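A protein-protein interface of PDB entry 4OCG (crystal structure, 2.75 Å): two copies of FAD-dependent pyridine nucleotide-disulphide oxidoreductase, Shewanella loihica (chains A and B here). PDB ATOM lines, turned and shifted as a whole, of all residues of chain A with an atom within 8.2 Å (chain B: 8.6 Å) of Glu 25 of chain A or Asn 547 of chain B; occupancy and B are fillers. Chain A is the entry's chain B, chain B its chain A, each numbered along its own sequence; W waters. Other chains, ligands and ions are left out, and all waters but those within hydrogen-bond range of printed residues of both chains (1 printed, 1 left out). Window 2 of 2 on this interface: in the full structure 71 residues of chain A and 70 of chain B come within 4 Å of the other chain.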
ATOM      1  N   LYS A   2      -6.763 -28.494   0.325  1.00  0.00           N
ATOM      2  CA  LYS A   2      -7.684 -29.619   0.065  1.00  0.00           C
ATOM      3  C   LYS A   2      -7.702 -30.082  -1.421  1.00  0.00           C
ATOM      4  O   LYS A   2      -7.878 -29.277  -2.334  1.00  0.00           O
ATOM      5  CB  LYS A   2      -9.080 -29.209   0.500  1.00  0.00           C
ATOM      6  CG  LYS A   2      -9.986 -30.344   0.871  1.00  0.00           C
ATOM      7  CD  LYS A   2     -10.870 -29.953   2.081  1.00  0.00           C
ATOM      8  CE  LYS A   2     -11.782 -31.108   2.449  1.00  0.00           C
ATOM      9  NZ  LYS A   2     -11.478 -31.737   3.754  1.00  0.00           N
ATOM     10  N   ALA A  20     -18.200 -26.076  -4.738  1.00  0.00           N
ATOM     11  CA  ALA A  20     -16.921 -26.237  -4.007  1.00  0.00           C
ATOM     12  C   ALA A  20     -15.972 -25.056  -4.243  1.00  0.00           C
ATOM     13  O   ALA A  20     -15.323 -24.593  -3.287  1.00  0.00           O
ATOM     14  CB  ALA A  20     -16.231 -27.579  -4.317  1.00  0.00           C
ATOM     15  N   ARG A  21     -15.911 -24.541  -5.481  1.00  0.00           N
ATOM     16  CA  ARG A  21     -15.105 -23.358  -5.742  1.00  0.00           C
ATOM     17  C   ARG A  21     -15.644 -22.122  -4.990  1.00  0.00           C
ATOM     18  O   ARG A  21     -14.895 -21.261  -4.576  1.00  0.00           O
ATOM     19  CB  ARG A  21     -15.053 -23.083  -7.236  1.00  0.00           C
ATOM     20  CG  ARG A  21     -14.102 -21.952  -7.659  1.00  0.00           C
ATOM     21  CD  ARG A  21     -12.720 -21.935  -6.969  1.00  0.00           C
ATOM     22  NE  ARG A  21     -11.779 -22.826  -7.626  1.00  0.00           N
ATOM     23  CZ  ARG A  21     -10.826 -23.553  -7.026  1.00  0.00           C
ATOM     24  NH1 ARG A  21     -10.632 -23.537  -5.704  1.00  0.00           N
ATOM     25  NH2 ARG A  21     -10.060 -24.339  -7.787  1.00  0.00           N
ATOM     26  N   ARG A  22     -16.955 -22.022  -4.843  1.00  0.00           N
ATOM     27  CA  ARG A  22     -17.540 -20.868  -4.174  1.00  0.00           C
ATOM     28  C   ARG A  22     -17.234 -20.885  -2.662  1.00  0.00           C
ATOM     29  O   ARG A  22     -17.256 -19.834  -1.983  1.00  0.00           O
ATOM     30  CB  ARG A  22     -19.043 -20.857  -4.399  1.00  0.00           C
ATOM     31  CG  ARG A  22     -19.395 -20.685  -5.832  1.00  0.00           C
ATOM     32  CD  ARG A  22     -20.790 -20.145  -5.948  1.00  0.00           C
ATOM     33  NE  ARG A  22     -21.761 -21.209  -5.785  1.00  0.00           N
ATOM     34  CZ  ARG A  22     -22.209 -21.963  -6.779  1.00  0.00           C
ATOM     35  NH1 ARG A  22     -21.759 -21.757  -7.989  1.00  0.00           N
ATOM     36  NH2 ARG A  22     -23.085 -22.931  -6.558  1.00  0.00           N
ATOM     37  N   LEU A  23     -16.945 -22.085  -2.148  1.00  0.00           N
ATOM     38  CA  LEU A  23     -16.615 -22.235  -0.755  1.00  0.00           C
ATOM     39  C   LEU A  23     -15.122 -22.007  -0.540  1.00  0.00           C
ATOM     40  O   LEU A  23     -14.744 -21.336   0.417  1.00  0.00           O
ATOM     41  CB  LEU A  23     -17.024 -23.613  -0.272  1.00  0.00           C
ATOM     42  CG  LEU A  23     -18.512 -23.886  -0.059  1.00  0.00           C
ATOM     43  CD1 LEU A  23     -18.818 -25.383   0.144  1.00  0.00           C
ATOM     44  CD2 LEU A  23     -18.943 -23.090   1.133  1.00  0.00           C
ATOM     45  N   SER A  24     -14.262 -22.557  -1.408  1.00  0.00           N
ATOM     46  CA  SER A  24     -12.808 -22.289  -1.304  1.00  0.00           C
ATOM     47  C   SER A  24     -12.120 -21.861  -2.597  1.00  0.00           C
ATOM     48  O   SER A  24     -12.373 -22.384  -3.670  1.00  0.00           O
ATOM     49  CB  SER A  24     -12.063 -23.439  -0.638  1.00  0.00           C
ATOM     50  OG  SER A  24     -10.793 -23.641  -1.240  1.00  0.00           O
ATOM     51  N   GLU A  25     -11.270 -20.866  -2.488  1.00  0.00           N
ATOM     52  CA  GLU A  25     -10.421 -20.510  -3.586  1.00  0.00           C
ATOM     53  C   GLU A  25      -9.132 -21.339  -3.544  1.00  0.00           C
ATOM     54  O   GLU A  25      -8.465 -21.424  -4.525  1.00  0.00           O
ATOM     55  CB  GLU A  25     -10.103 -19.000  -3.579  1.00  0.00           C
ATOM     56  CG  GLU A  25     -11.096 -18.072  -4.311  1.00  0.00           C
ATOM     57  CD  GLU A  25     -11.248 -18.432  -5.789  1.00  0.00           C
ATOM     58  OE1 GLU A  25     -10.218 -18.472  -6.546  1.00  0.00           O
ATOM     59  OE2 GLU A  25     -12.406 -18.704  -6.171  1.00  0.00           O
ATOM     60  N   THR A  26      -8.771 -21.946  -2.425  1.00  0.00           N
ATOM     61  CA  THR A  26      -7.477 -22.631  -2.353  1.00  0.00           C
ATOM     62  C   THR A  26      -7.506 -24.099  -2.758  1.00  0.00           C
ATOM     63  O   THR A  26      -6.462 -24.671  -3.020  1.00  0.00           O
ATOM     64  CB  THR A  26      -6.867 -22.650  -0.918  1.00  0.00           C
ATOM     65  OG1 THR A  26      -7.780 -23.310  -0.016  1.00  0.00           O
ATOM     66  CG2 THR A  26      -6.433 -21.241  -0.425  1.00  0.00           C
ATOM     67  N   ALA A  27      -8.672 -24.731  -2.748  1.00  0.00           N
ATOM     68  CA  ALA A  27      -8.734 -26.141  -3.119  1.00  0.00           C
ATOM     69  C   ALA A  27      -8.399 -26.414  -4.601  1.00  0.00           C
ATOM     70  O   ALA A  27      -8.851 -25.687  -5.489  1.00  0.00           O
ATOM     71  CB  ALA A  27     -10.078 -26.657  -2.814  1.00  0.00           C
ATOM     72  N   GLU A  28      -7.635 -27.477  -4.857  1.00  0.00           N
ATOM     73  CA  GLU A  28      -7.553 -28.072  -6.186  1.00  0.00           C
ATOM     74  C   GLU A  28      -8.824 -28.800  -6.466  1.00  0.00           C
ATOM     75  O   GLU A  28      -9.207 -29.668  -5.666  1.00  0.00           O
ATOM     76  CB  GLU A  28      -6.435 -29.108  -6.258  1.00  0.00           C
ATOM     77  CG  GLU A  28      -5.199 -28.661  -7.087  1.00  0.00           C
ATOM     78  CD  GLU A  28      -4.496 -29.831  -7.797  1.00  0.00           C
ATOM     79  OE1 GLU A  28      -4.063 -30.792  -7.108  1.00  0.00           O
ATOM     80  OE2 GLU A  28      -4.381 -29.778  -9.055  1.00  0.00           O
ATOM     81  N   ILE A  29      -9.459 -28.509  -7.602  1.00  0.00           N
ATOM     82  CA  ILE A  29     -10.623 -29.305  -8.021  1.00  0.00           C
ATOM     83  C   ILE A  29     -10.451 -29.895  -9.427  1.00  0.00           C
ATOM     84  O   ILE A  29     -10.367 -29.146 -10.397  1.00  0.00           O
ATOM     85  CB  ILE A  29     -11.956 -28.485  -7.991  1.00  0.00           C
ATOM     86  CG1 ILE A  29     -12.233 -27.902  -6.601  1.00  0.00           C
ATOM     87  CG2 ILE A  29     -13.148 -29.372  -8.421  1.00  0.00           C
ATOM     88  CD1 ILE A  29     -12.956 -26.583  -6.598  1.00  0.00           C
ATOM     89  N   ARG A  70     -14.411 -19.647 -15.129  1.00  0.00           N
ATOM     90  CA  ARG A  70     -15.294 -19.114 -14.087  1.00  0.00           C
ATOM     91  C   ARG A  70     -14.950 -19.691 -12.743  1.00  0.00           C
ATOM     92  O   ARG A  70     -14.828 -18.939 -11.775  1.00  0.00           O
ATOM     93  CB  ARG A  70     -16.794 -19.258 -14.397  1.00  0.00           C
ATOM     94  CG  ARG A  70     -17.742 -18.866 -13.227  1.00  0.00           C
ATOM     95  CD  ARG A  70     -19.206 -18.631 -13.684  1.00  0.00           C
ATOM     96  NE  ARG A  70     -19.293 -17.692 -14.828  1.00  0.00           N
ATOM     97  CZ  ARG A  70     -20.387 -17.413 -15.536  1.00  0.00           C
ATOM     98  NH1 ARG A  70     -21.547 -17.978 -15.243  1.00  0.00           N
ATOM     99  NH2 ARG A  70     -20.329 -16.520 -16.509  1.00  0.00           N
ATOM    100  N   PHE A  71     -14.763 -21.008 -12.688  1.00  0.00           N
ATOM    101  CA  PHE A  71     -14.567 -21.713 -11.409  1.00  0.00           C
ATOM    102  C   PHE A  71     -13.165 -22.328 -11.154  1.00  0.00           C
ATOM    103  O   PHE A  71     -12.937 -22.913 -10.089  1.00  0.00           O
ATOM    104  CB  PHE A  71     -15.658 -22.774 -11.247  1.00  0.00           C
ATOM    105  CG  PHE A  71     -17.038 -22.207 -11.192  1.00  0.00           C
ATOM    106  CD1 PHE A  71     -17.416 -21.375 -10.144  1.00  0.00           C
ATOM    107  CD2 PHE A  71     -17.957 -22.479 -12.208  1.00  0.00           C
ATOM    108  CE1 PHE A  71     -18.664 -20.837 -10.091  1.00  0.00           C
ATOM    109  CE2 PHE A  71     -19.201 -21.952 -12.189  1.00  0.00           C
ATOM    110  CZ  PHE A  71     -19.576 -21.138 -11.117  1.00  0.00           C
ATOM    111  N   ASN A  72     -12.235 -22.197 -12.106  1.00  0.00           N
ATOM    112  CA  ASN A  72     -10.879 -22.729 -11.946  1.00  0.00           C
ATOM    113  C   ASN A  72     -10.865 -24.165 -11.427  1.00  0.00           C
ATOM    114  O   ASN A  72     -10.123 -24.530 -10.500  1.00  0.00           O
ATOM    115  CB  ASN A  72      -9.973 -21.822 -11.099  1.00  0.00           C
ATOM    116  CG  ASN A  72      -8.523 -22.343 -11.027  1.00  0.00           C
ATOM    117  OD1 ASN A  72      -7.981 -22.996 -11.991  1.00  0.00           O
ATOM    118  ND2 ASN A  72      -7.883 -22.074  -9.895  1.00  0.00           N
ATOM    119  N   PHE A 336     -16.276 -29.674   3.038  1.00  0.00           N
ATOM    120  CA  PHE A 336     -15.725 -28.603   3.885  1.00  0.00           C
ATOM    121  C   PHE A 336     -16.211 -28.596   5.345  1.00  0.00           C
ATOM    122  O   PHE A 336     -16.332 -27.545   5.976  1.00  0.00           O
ATOM    123  CB  PHE A 336     -15.904 -27.260   3.192  1.00  0.00           C
ATOM    124  CG  PHE A 336     -15.099 -27.164   1.948  1.00  0.00           C
ATOM    125  CD1 PHE A 336     -13.801 -26.646   1.980  1.00  0.00           C
ATOM    126  CD2 PHE A 336     -15.585 -27.671   0.751  1.00  0.00           C
ATOM    127  CE1 PHE A 336     -13.022 -26.591   0.825  1.00  0.00           C
ATOM    128  CE2 PHE A 336     -14.803 -27.620  -0.422  1.00  0.00           C
ATOM    129  CZ  PHE A 336     -13.528 -27.081  -0.375  1.00  0.00           C
ATOM    130  N   LEU B 514     -11.936 -12.550 -13.633  1.00  0.00           N
ATOM    131  CA  LEU B 514     -11.638 -11.920 -12.377  1.00  0.00           C
ATOM    132  C   LEU B 514     -10.531 -12.555 -11.627  1.00  0.00           C
ATOM    133  O   LEU B 514      -9.720 -11.885 -11.063  1.00  0.00           O
ATOM    134  CB  LEU B 514     -12.871 -11.915 -11.511  1.00  0.00           C
ATOM    135  CG  LEU B 514     -12.761 -11.133 -10.229  1.00  0.00           C
ATOM    136  CD1 LEU B 514     -12.746  -9.715 -10.517  1.00  0.00           C
ATOM    137  CD2 LEU B 514     -13.895 -11.444  -9.362  1.00  0.00           C
ATOM    138  N   ARG B 515     -10.516 -13.864 -11.602  1.00  0.00           N
ATOM    139  CA  ARG B 515      -9.524 -14.578 -10.862  1.00  0.00           C
ATOM    140  C   ARG B 515      -8.179 -14.168 -11.321  1.00  0.00           C
ATOM    141  O   ARG B 515      -7.268 -14.095 -10.561  1.00  0.00           O
ATOM    142  CB  ARG B 515      -9.693 -16.055 -11.085  1.00  0.00           C
ATOM    143  CG  ARG B 515      -8.846 -16.918 -10.242  1.00  0.00           C
ATOM    144  CD  ARG B 515      -9.291 -18.305 -10.324  1.00  0.00           C
ATOM    145  NE  ARG B 515     -10.491 -18.516  -9.568  1.00  0.00           N
ATOM    146  CZ  ARG B 515     -11.668 -18.712 -10.104  1.00  0.00           C
ATOM    147  NH1 ARG B 515     -11.795 -18.735 -11.394  1.00  0.00           N
ATOM    148  NH2 ARG B 515     -12.702 -18.867  -9.345  1.00  0.00           N
ATOM    149  N   ASP B 516      -8.068 -13.887 -12.591  1.00  0.00           N
ATOM    150  CA  ASP B 516      -6.796 -13.629 -13.173  1.00  0.00           C
ATOM    151  C   ASP B 516      -6.434 -12.183 -12.988  1.00  0.00           C
ATOM    152  O   ASP B 516      -5.293 -11.834 -12.901  1.00  0.00           O
ATOM    153  CB  ASP B 516      -6.839 -13.989 -14.640  1.00  0.00           C
ATOM    154  CG  ASP B 516      -6.723 -15.482 -14.888  1.00  0.00           C
ATOM    155  OD1 ASP B 516      -6.191 -16.212 -14.051  1.00  0.00           O
ATOM    156  OD2 ASP B 516      -7.154 -15.936 -15.956  1.00  0.00           O
ATOM    157  N   MET B 518      -7.644 -10.133 -10.419  1.00  0.00           N
ATOM    158  CA  MET B 518      -7.975  -9.684  -9.085  1.00  0.00           C
ATOM    159  C   MET B 518      -7.067  -8.555  -8.558  1.00  0.00           C
ATOM    160  O   MET B 518      -7.541  -7.657  -7.842  1.00  0.00           O
ATOM    161  CB  MET B 518      -7.934 -10.872  -8.133  1.00  0.00           C
ATOM    162  CG  MET B 518      -8.394 -10.522  -6.759  1.00  0.00           C
ATOM    163  SD  MET B 518      -9.633 -11.666  -6.185  1.00  0.00           S
ATOM    164  CE  MET B 518      -8.701 -13.183  -6.031  1.00  0.00           C
ATOM    165  N   LYS B 523      -7.318  -4.237  -2.116  1.00  0.00           N
ATOM    166  CA  LYS B 523      -7.788  -4.859  -0.880  1.00  0.00           C
ATOM    167  C   LYS B 523      -8.180  -3.821   0.227  1.00  0.00           C
ATOM    168  O   LYS B 523      -8.850  -4.164   1.199  1.00  0.00           O
ATOM    169  CB  LYS B 523      -6.735  -5.873  -0.423  1.00  0.00           C
ATOM    170  CG  LYS B 523      -7.274  -7.260  -0.035  1.00  0.00           C
ATOM    171  CD  LYS B 523      -6.394  -8.395  -0.582  1.00  0.00           C
ATOM    172  CE  LYS B 523      -6.238  -9.533   0.427  1.00  0.00           C
ATOM    173  NZ  LYS B 523      -5.638 -10.777  -0.185  1.00  0.00           N
ATOM    174  N   VAL B 539     -20.922 -15.237  -7.656  1.00  0.00           N
ATOM    175  CA  VAL B 539     -19.623 -15.862  -8.001  1.00  0.00           C
ATOM    176  C   VAL B 539     -18.415 -14.943  -7.652  1.00  0.00           C
ATOM    177  O   VAL B 539     -17.467 -15.355  -6.973  1.00  0.00           O
ATOM    178  CB  VAL B 539     -19.543 -16.319  -9.500  1.00  0.00           C
ATOM    179  CG1 VAL B 539     -18.255 -17.007  -9.758  1.00  0.00           C
ATOM    180  CG2 VAL B 539     -20.732 -17.250  -9.904  1.00  0.00           C
ATOM    181  N   ALA B 540     -18.483 -13.695  -8.102  1.00  0.00           N
ATOM    182  CA  ALA B 540     -17.482 -12.665  -7.796  1.00  0.00           C
ATOM    183  C   ALA B 540     -17.289 -12.409  -6.301  1.00  0.00           C
ATOM    184  O   ALA B 540     -16.146 -12.287  -5.807  1.00  0.00           O
ATOM    185  CB  ALA B 540     -17.899 -11.368  -8.455  1.00  0.00           C
ATOM    186  N   TYR B 541     -18.407 -12.240  -5.591  1.00  0.00           N
ATOM    187  CA  TYR B 541     -18.350 -12.051  -4.169  1.00  0.00           C
ATOM    188  C   TYR B 541     -17.615 -13.197  -3.502  1.00  0.00           C
ATOM    189  O   TYR B 541     -16.932 -12.958  -2.531  1.00  0.00           O
ATOM    190  CB  TYR B 541     -19.747 -11.972  -3.581  1.00  0.00           C
ATOM    191  CG  TYR B 541     -19.799 -12.006  -2.065  1.00  0.00           C
ATOM    192  CD1 TYR B 541     -19.724 -10.835  -1.323  1.00  0.00           C
ATOM    193  CD2 TYR B 541     -19.936 -13.196  -1.379  1.00  0.00           C
ATOM    194  CE1 TYR B 541     -19.785 -10.838   0.095  1.00  0.00           C
ATOM    195  CE2 TYR B 541     -20.001 -13.220   0.043  1.00  0.00           C
ATOM    196  CZ  TYR B 541     -19.930 -12.025   0.754  1.00  0.00           C
ATOM    197  OH  TYR B 541     -19.990 -12.024   2.125  1.00  0.00           O
ATOM    198  N   ARG B 542     -17.784 -14.430  -3.983  1.00  0.00           N
ATOM    199  CA  ARG B 542     -17.164 -15.557  -3.314  1.00  0.00           C
ATOM    200  C   ARG B 542     -15.678 -15.556  -3.641  1.00  0.00           C
ATOM    201  O   ARG B 542     -14.842 -15.709  -2.736  1.00  0.00           O
ATOM    202  CB  ARG B 542     -17.820 -16.871  -3.688  1.00  0.00           C
ATOM    203  CG  ARG B 542     -19.269 -16.984  -3.227  1.00  0.00           C
ATOM    204  CD  ARG B 542     -19.451 -16.945  -1.689  1.00  0.00           C
ATOM    205  NE  ARG B 542     -18.334 -17.580  -1.046  1.00  0.00           N
ATOM    206  CZ  ARG B 542     -18.183 -17.732   0.263  1.00  0.00           C
ATOM    207  NH1 ARG B 542     -19.092 -17.293   1.120  1.00  0.00           N
ATOM    208  NH2 ARG B 542     -17.096 -18.334   0.722  1.00  0.00           N
ATOM    209  N   GLN B 543     -15.340 -15.321  -4.907  1.00  0.00           N
ATOM    210  CA  GLN B 543     -13.938 -15.179  -5.272  1.00  0.00           C
ATOM    211  C   GLN B 543     -13.198 -14.199  -4.339  1.00  0.00           C
ATOM    212  O   GLN B 543     -12.104 -14.492  -3.823  1.00  0.00           O
ATOM    213  CB  GLN B 543     -13.783 -14.797  -6.736  1.00  0.00           C
ATOM    214  CG  GLN B 543     -14.170 -15.932  -7.635  1.00  0.00           C
ATOM    215  CD  GLN B 543     -13.674 -15.781  -9.072  1.00  0.00           C
ATOM    216  OE1 GLN B 543     -14.101 -16.513  -9.951  1.00  0.00           O
ATOM    217  NE2 GLN B 543     -12.774 -14.855  -9.310  1.00  0.00           N
ATOM    218  N   LEU B 544     -13.852 -13.074  -4.088  1.00  0.00           N
ATOM    219  CA  LEU B 544     -13.251 -11.954  -3.370  1.00  0.00           C
ATOM    220  C   LEU B 544     -13.132 -12.183  -1.869  1.00  0.00           C
ATOM    221  O   LEU B 544     -12.006 -12.069  -1.336  1.00  0.00           O
ATOM    222  CB  LEU B 544     -13.996 -10.646  -3.669  1.00  0.00           C
ATOM    223  CG  LEU B 544     -13.784 -10.029  -5.062  1.00  0.00           C
ATOM    224  CD1 LEU B 544     -14.366  -8.714  -5.080  1.00  0.00           C
ATOM    225  CD2 LEU B 544     -12.316  -9.886  -5.454  1.00  0.00           C
ATOM    226  N   VAL B 545     -14.242 -12.501  -1.183  1.00  0.00           N
ATOM    227  CA  VAL B 545     -14.144 -12.765   0.256  1.00  0.00           C
ATOM    228  C   VAL B 545     -13.155 -13.898   0.427  1.00  0.00           C
ATOM    229  O   VAL B 545     -12.251 -13.799   1.257  1.00  0.00           O
ATOM    230  CB  VAL B 545     -15.472 -13.050   1.009  1.00  0.00           C
ATOM    231  CG1 VAL B 545     -16.449 -11.910   0.830  1.00  0.00           C
ATOM    232  CG2 VAL B 545     -16.089 -14.332   0.580  1.00  0.00           C
ATOM    233  N   ASN B 546     -13.249 -14.927  -0.417  1.00  0.00           N
ATOM    234  CA  ASN B 546     -12.304 -16.023  -0.283  1.00  0.00           C
ATOM    235  C   ASN B 546     -10.853 -15.579  -0.298  1.00  0.00           C
ATOM    236  O   ASN B 546     -10.027 -16.226   0.310  1.00  0.00           O
ATOM    237  CB  ASN B 546     -12.558 -17.115  -1.304  1.00  0.00           C
ATOM    238  CG  ASN B 546     -13.740 -17.994  -0.937  1.00  0.00           C
ATOM    239  OD1 ASN B 546     -14.337 -18.668  -1.806  1.00  0.00           O
ATOM    240  ND2 ASN B 546     -14.095 -17.995   0.351  1.00  0.00           N
ATOM    241  N   ASN B 547     -10.548 -14.472  -0.972  1.00  0.00           N
ATOM    242  CA  ASN B 547      -9.196 -13.890  -0.964  1.00  0.00           C
ATOM    243  C   ASN B 547      -9.035 -12.735   0.035  1.00  0.00           C
ATOM    244  O   ASN B 547      -8.073 -11.969  -0.028  1.00  0.00           O
ATOM    245  CB  ASN B 547      -8.802 -13.449  -2.354  1.00  0.00           C
ATOM    246  CG  ASN B 547      -8.289 -14.588  -3.172  1.00  0.00           C
ATOM    247  OD1 ASN B 547      -8.999 -15.125  -4.008  1.00  0.00           O
ATOM    248  ND2 ASN B 547      -7.053 -14.991  -2.929  1.00  0.00           N
ATOM    249  N   GLY B 548      -9.994 -12.606   0.948  1.00  0.00           N
ATOM    250  CA  GLY B 548      -9.867 -11.686   2.056  1.00  0.00           C
ATOM    251  C   GLY B 548     -10.256 -10.260   1.741  1.00  0.00           C
ATOM    252  O   GLY B 548      -9.838  -9.336   2.423  1.00  0.00           O
ATOM    253  N   TYR B 549     -11.065 -10.067   0.714  1.00  0.00           N
ATOM    254  CA  TYR B 549     -11.616  -8.755   0.444  1.00  0.00           C
ATOM    255  C   TYR B 549     -12.873  -8.611   1.270  1.00  0.00           C
ATOM    256  O   TYR B 549     -13.559  -9.616   1.499  1.00  0.00           O
ATOM    257  CB  TYR B 549     -12.004  -8.690  -1.015  1.00  0.00           C
ATOM    258  CG  TYR B 549     -10.864  -8.431  -1.962  1.00  0.00           C
ATOM    259  CD1 TYR B 549     -10.204  -9.466  -2.599  1.00  0.00           C
ATOM    260  CD2 TYR B 549     -10.481  -7.133  -2.259  1.00  0.00           C
ATOM    261  CE1 TYR B 549      -9.176  -9.203  -3.488  1.00  0.00           C
ATOM    262  CE2 TYR B 549      -9.445  -6.871  -3.138  1.00  0.00           C
ATOM    263  CZ  TYR B 549      -8.793  -7.892  -3.741  1.00  0.00           C
ATOM    264  OH  TYR B 549      -7.771  -7.573  -4.616  1.00  0.00           O
ATOM    265  N   ARG B 550     -13.187  -7.396   1.723  1.00  0.00           N
ATOM    266  CA  ARG B 550     -14.574  -7.113   2.184  1.00  0.00           C
ATOM    267  C   ARG B 550     -15.389  -6.875   0.896  1.00  0.00           C
ATOM    268  O   ARG B 550     -14.900  -6.259  -0.056  1.00  0.00           O
ATOM    269  CB  ARG B 550     -14.657  -5.907   3.157  1.00  0.00           C
ATOM    270  CG  ARG B 550     -13.388  -5.714   4.057  1.00  0.00           C
ATOM    271  CD  ARG B 550     -13.543  -4.781   5.290  1.00  0.00           C
ATOM    272  NE  ARG B 550     -14.056  -3.429   4.988  1.00  0.00           N
ATOM    273  CZ  ARG B 550     -13.368  -2.482   4.343  1.00  0.00           C
ATOM    274  NH1 ARG B 550     -12.140  -2.736   3.911  1.00  0.00           N
ATOM    275  NH2 ARG B 550     -13.913  -1.294   4.094  1.00  0.00           N
HETATM  276  O   HOH W   1     -10.200 -19.408  -0.215  1.00  0.00           O
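The guanidinium group (NE) of Arg 515 of chain B lies within salt-bridge range of the side-chain carboxylate (OE1) of Glu 25 of chain A. The guanidinium group (NH1) of Arg 515 of chain B lies within hydrogen-bond range of the backbone carbonyl oxygen (O) of Arg 70 of chain A, 3.1 Å away. The guanidinium group of Arg 542 of chain B sits at hydrogen-bond distance from the backbone carbonyl oxygen of Arg 22 of chain A (2.7 Å). The backbone carbonyl oxygen of Arg 70 of chain A lies close to the side-chain amide oxygen of Gln 543 of chain B, at 3.1 Å. OD1 of Asn 546 of chain B sits close to O of Arg 22 of chain A, at 3.1 Å. The side-chain amide nitrogen (ND2) of Asn 546 of chain B sits at hydrogen-bond distance from the backbone carbonyl oxygen (O) of Leu 23 of chain A (3.4 Å).
The backbone carbonyl oxygen of Asn 547 of chain B lies within hydrogen-bond range of the side-chain amino group of Lys 523 of chain B, at 2.7 Å. OD1 of Asn 547 of chain B lies close to O of Gln 543 of chain B, at 3.2 Å. NH1 of Arg 21 of chain A lies within hydrogen-bond range of O of Ser 24 of chain A (2.9 Å). NH1 of Arg 21 of chain A lies within hydrogen-bond range of O of Glu 25 of chain A (3.2 Å). The backbone carbonyl oxygen (O) of Asn 72 of chain A is in hydrogen-bond range of the guanidinium group (NH2) of Arg 21 of chain A (2.7 Å). The side-chain hydroxyl (OG) of Ser 24 of chain A sits at hydrogen-bond distance from the backbone NH (N) of Thr 26 of chain A, at 2.9 Å.
Water W1 lies within hydrogen-bond range of N of Glu 25 of chain A and O of Asn 546 of chain B.
Asn 547 of chain B touches one residue of chain A. No residue of chain B comes within 4 Å of Thr 26 of chain A. No residue of chain A comes within 4 Å of Gly 548 of chain B. Printed residues of chain A within 4 Å of Arg 542 of chain B: Arg 22 (2.7 Å) and Leu 23 (3.8 Å). Printed residues of chain B within 4 Å of Leu 23 of chain A: Arg 542 and Asn 546. Of the printed residues of chain A, Asn 546 of chain B touches Arg 21, Arg 22, Leu 23, Ser 24 and Glu 25. Phe 336 of chain A touches none of the printed residues of chain B. The nearest residue of chain B that does not touch Glu 25 of chain A is Arg 542 of chain B (4.7 Å). The nearest residue of chain A that does not touch Asn 547 of chain B is Thr 26 of chain A (6.8 Å). The nearest printed residue of chain A that does not touch Asn 546 of chain B is Ala 20 of chain A (6.2 Å).
Of the 17 printed residues of chain B, 6 touch a printed residue of chain A. Among the printed residues, Asp or Glu carboxylates within 4 Å of a Lys or Arg side-chain nitrogen of the other chain: Glu 25 of chain A with Arg 515 of chain B (3.0 Å).
No position is printed for both chains.
Arg 21 of chain A touches Arg 515 of chain B. Arg 21 of chain A touches Asn 546 of chain B (O to OD1, 3.8 Å). Leu 23 of chain A touches Arg 542 of chain B. Asn 546 of chain B touches Ser 24 of chain A (OD1 to N, 3.9 Å). OE2 of Glu 25 of chain A touches CG of Gln 543 of chain B, 3.6 Å away. Asn 546 of chain B touches Glu 25 of chain A (CB to CG, 3.5 Å). OD1 of Asn 547 of chain B touches CG of Glu 25 of chain A, 3.6 Å away. Val 539 of chain B touches Arg 70 of chain A (CG1 to CG, 3.97 Å). Val 539 of chain B touches Phe 71 of chain A (CG1 to CE1, 3.9 Å). N of Asn 72 of chain A touches NH1 of Arg 515 of chain B (3.6 Å).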
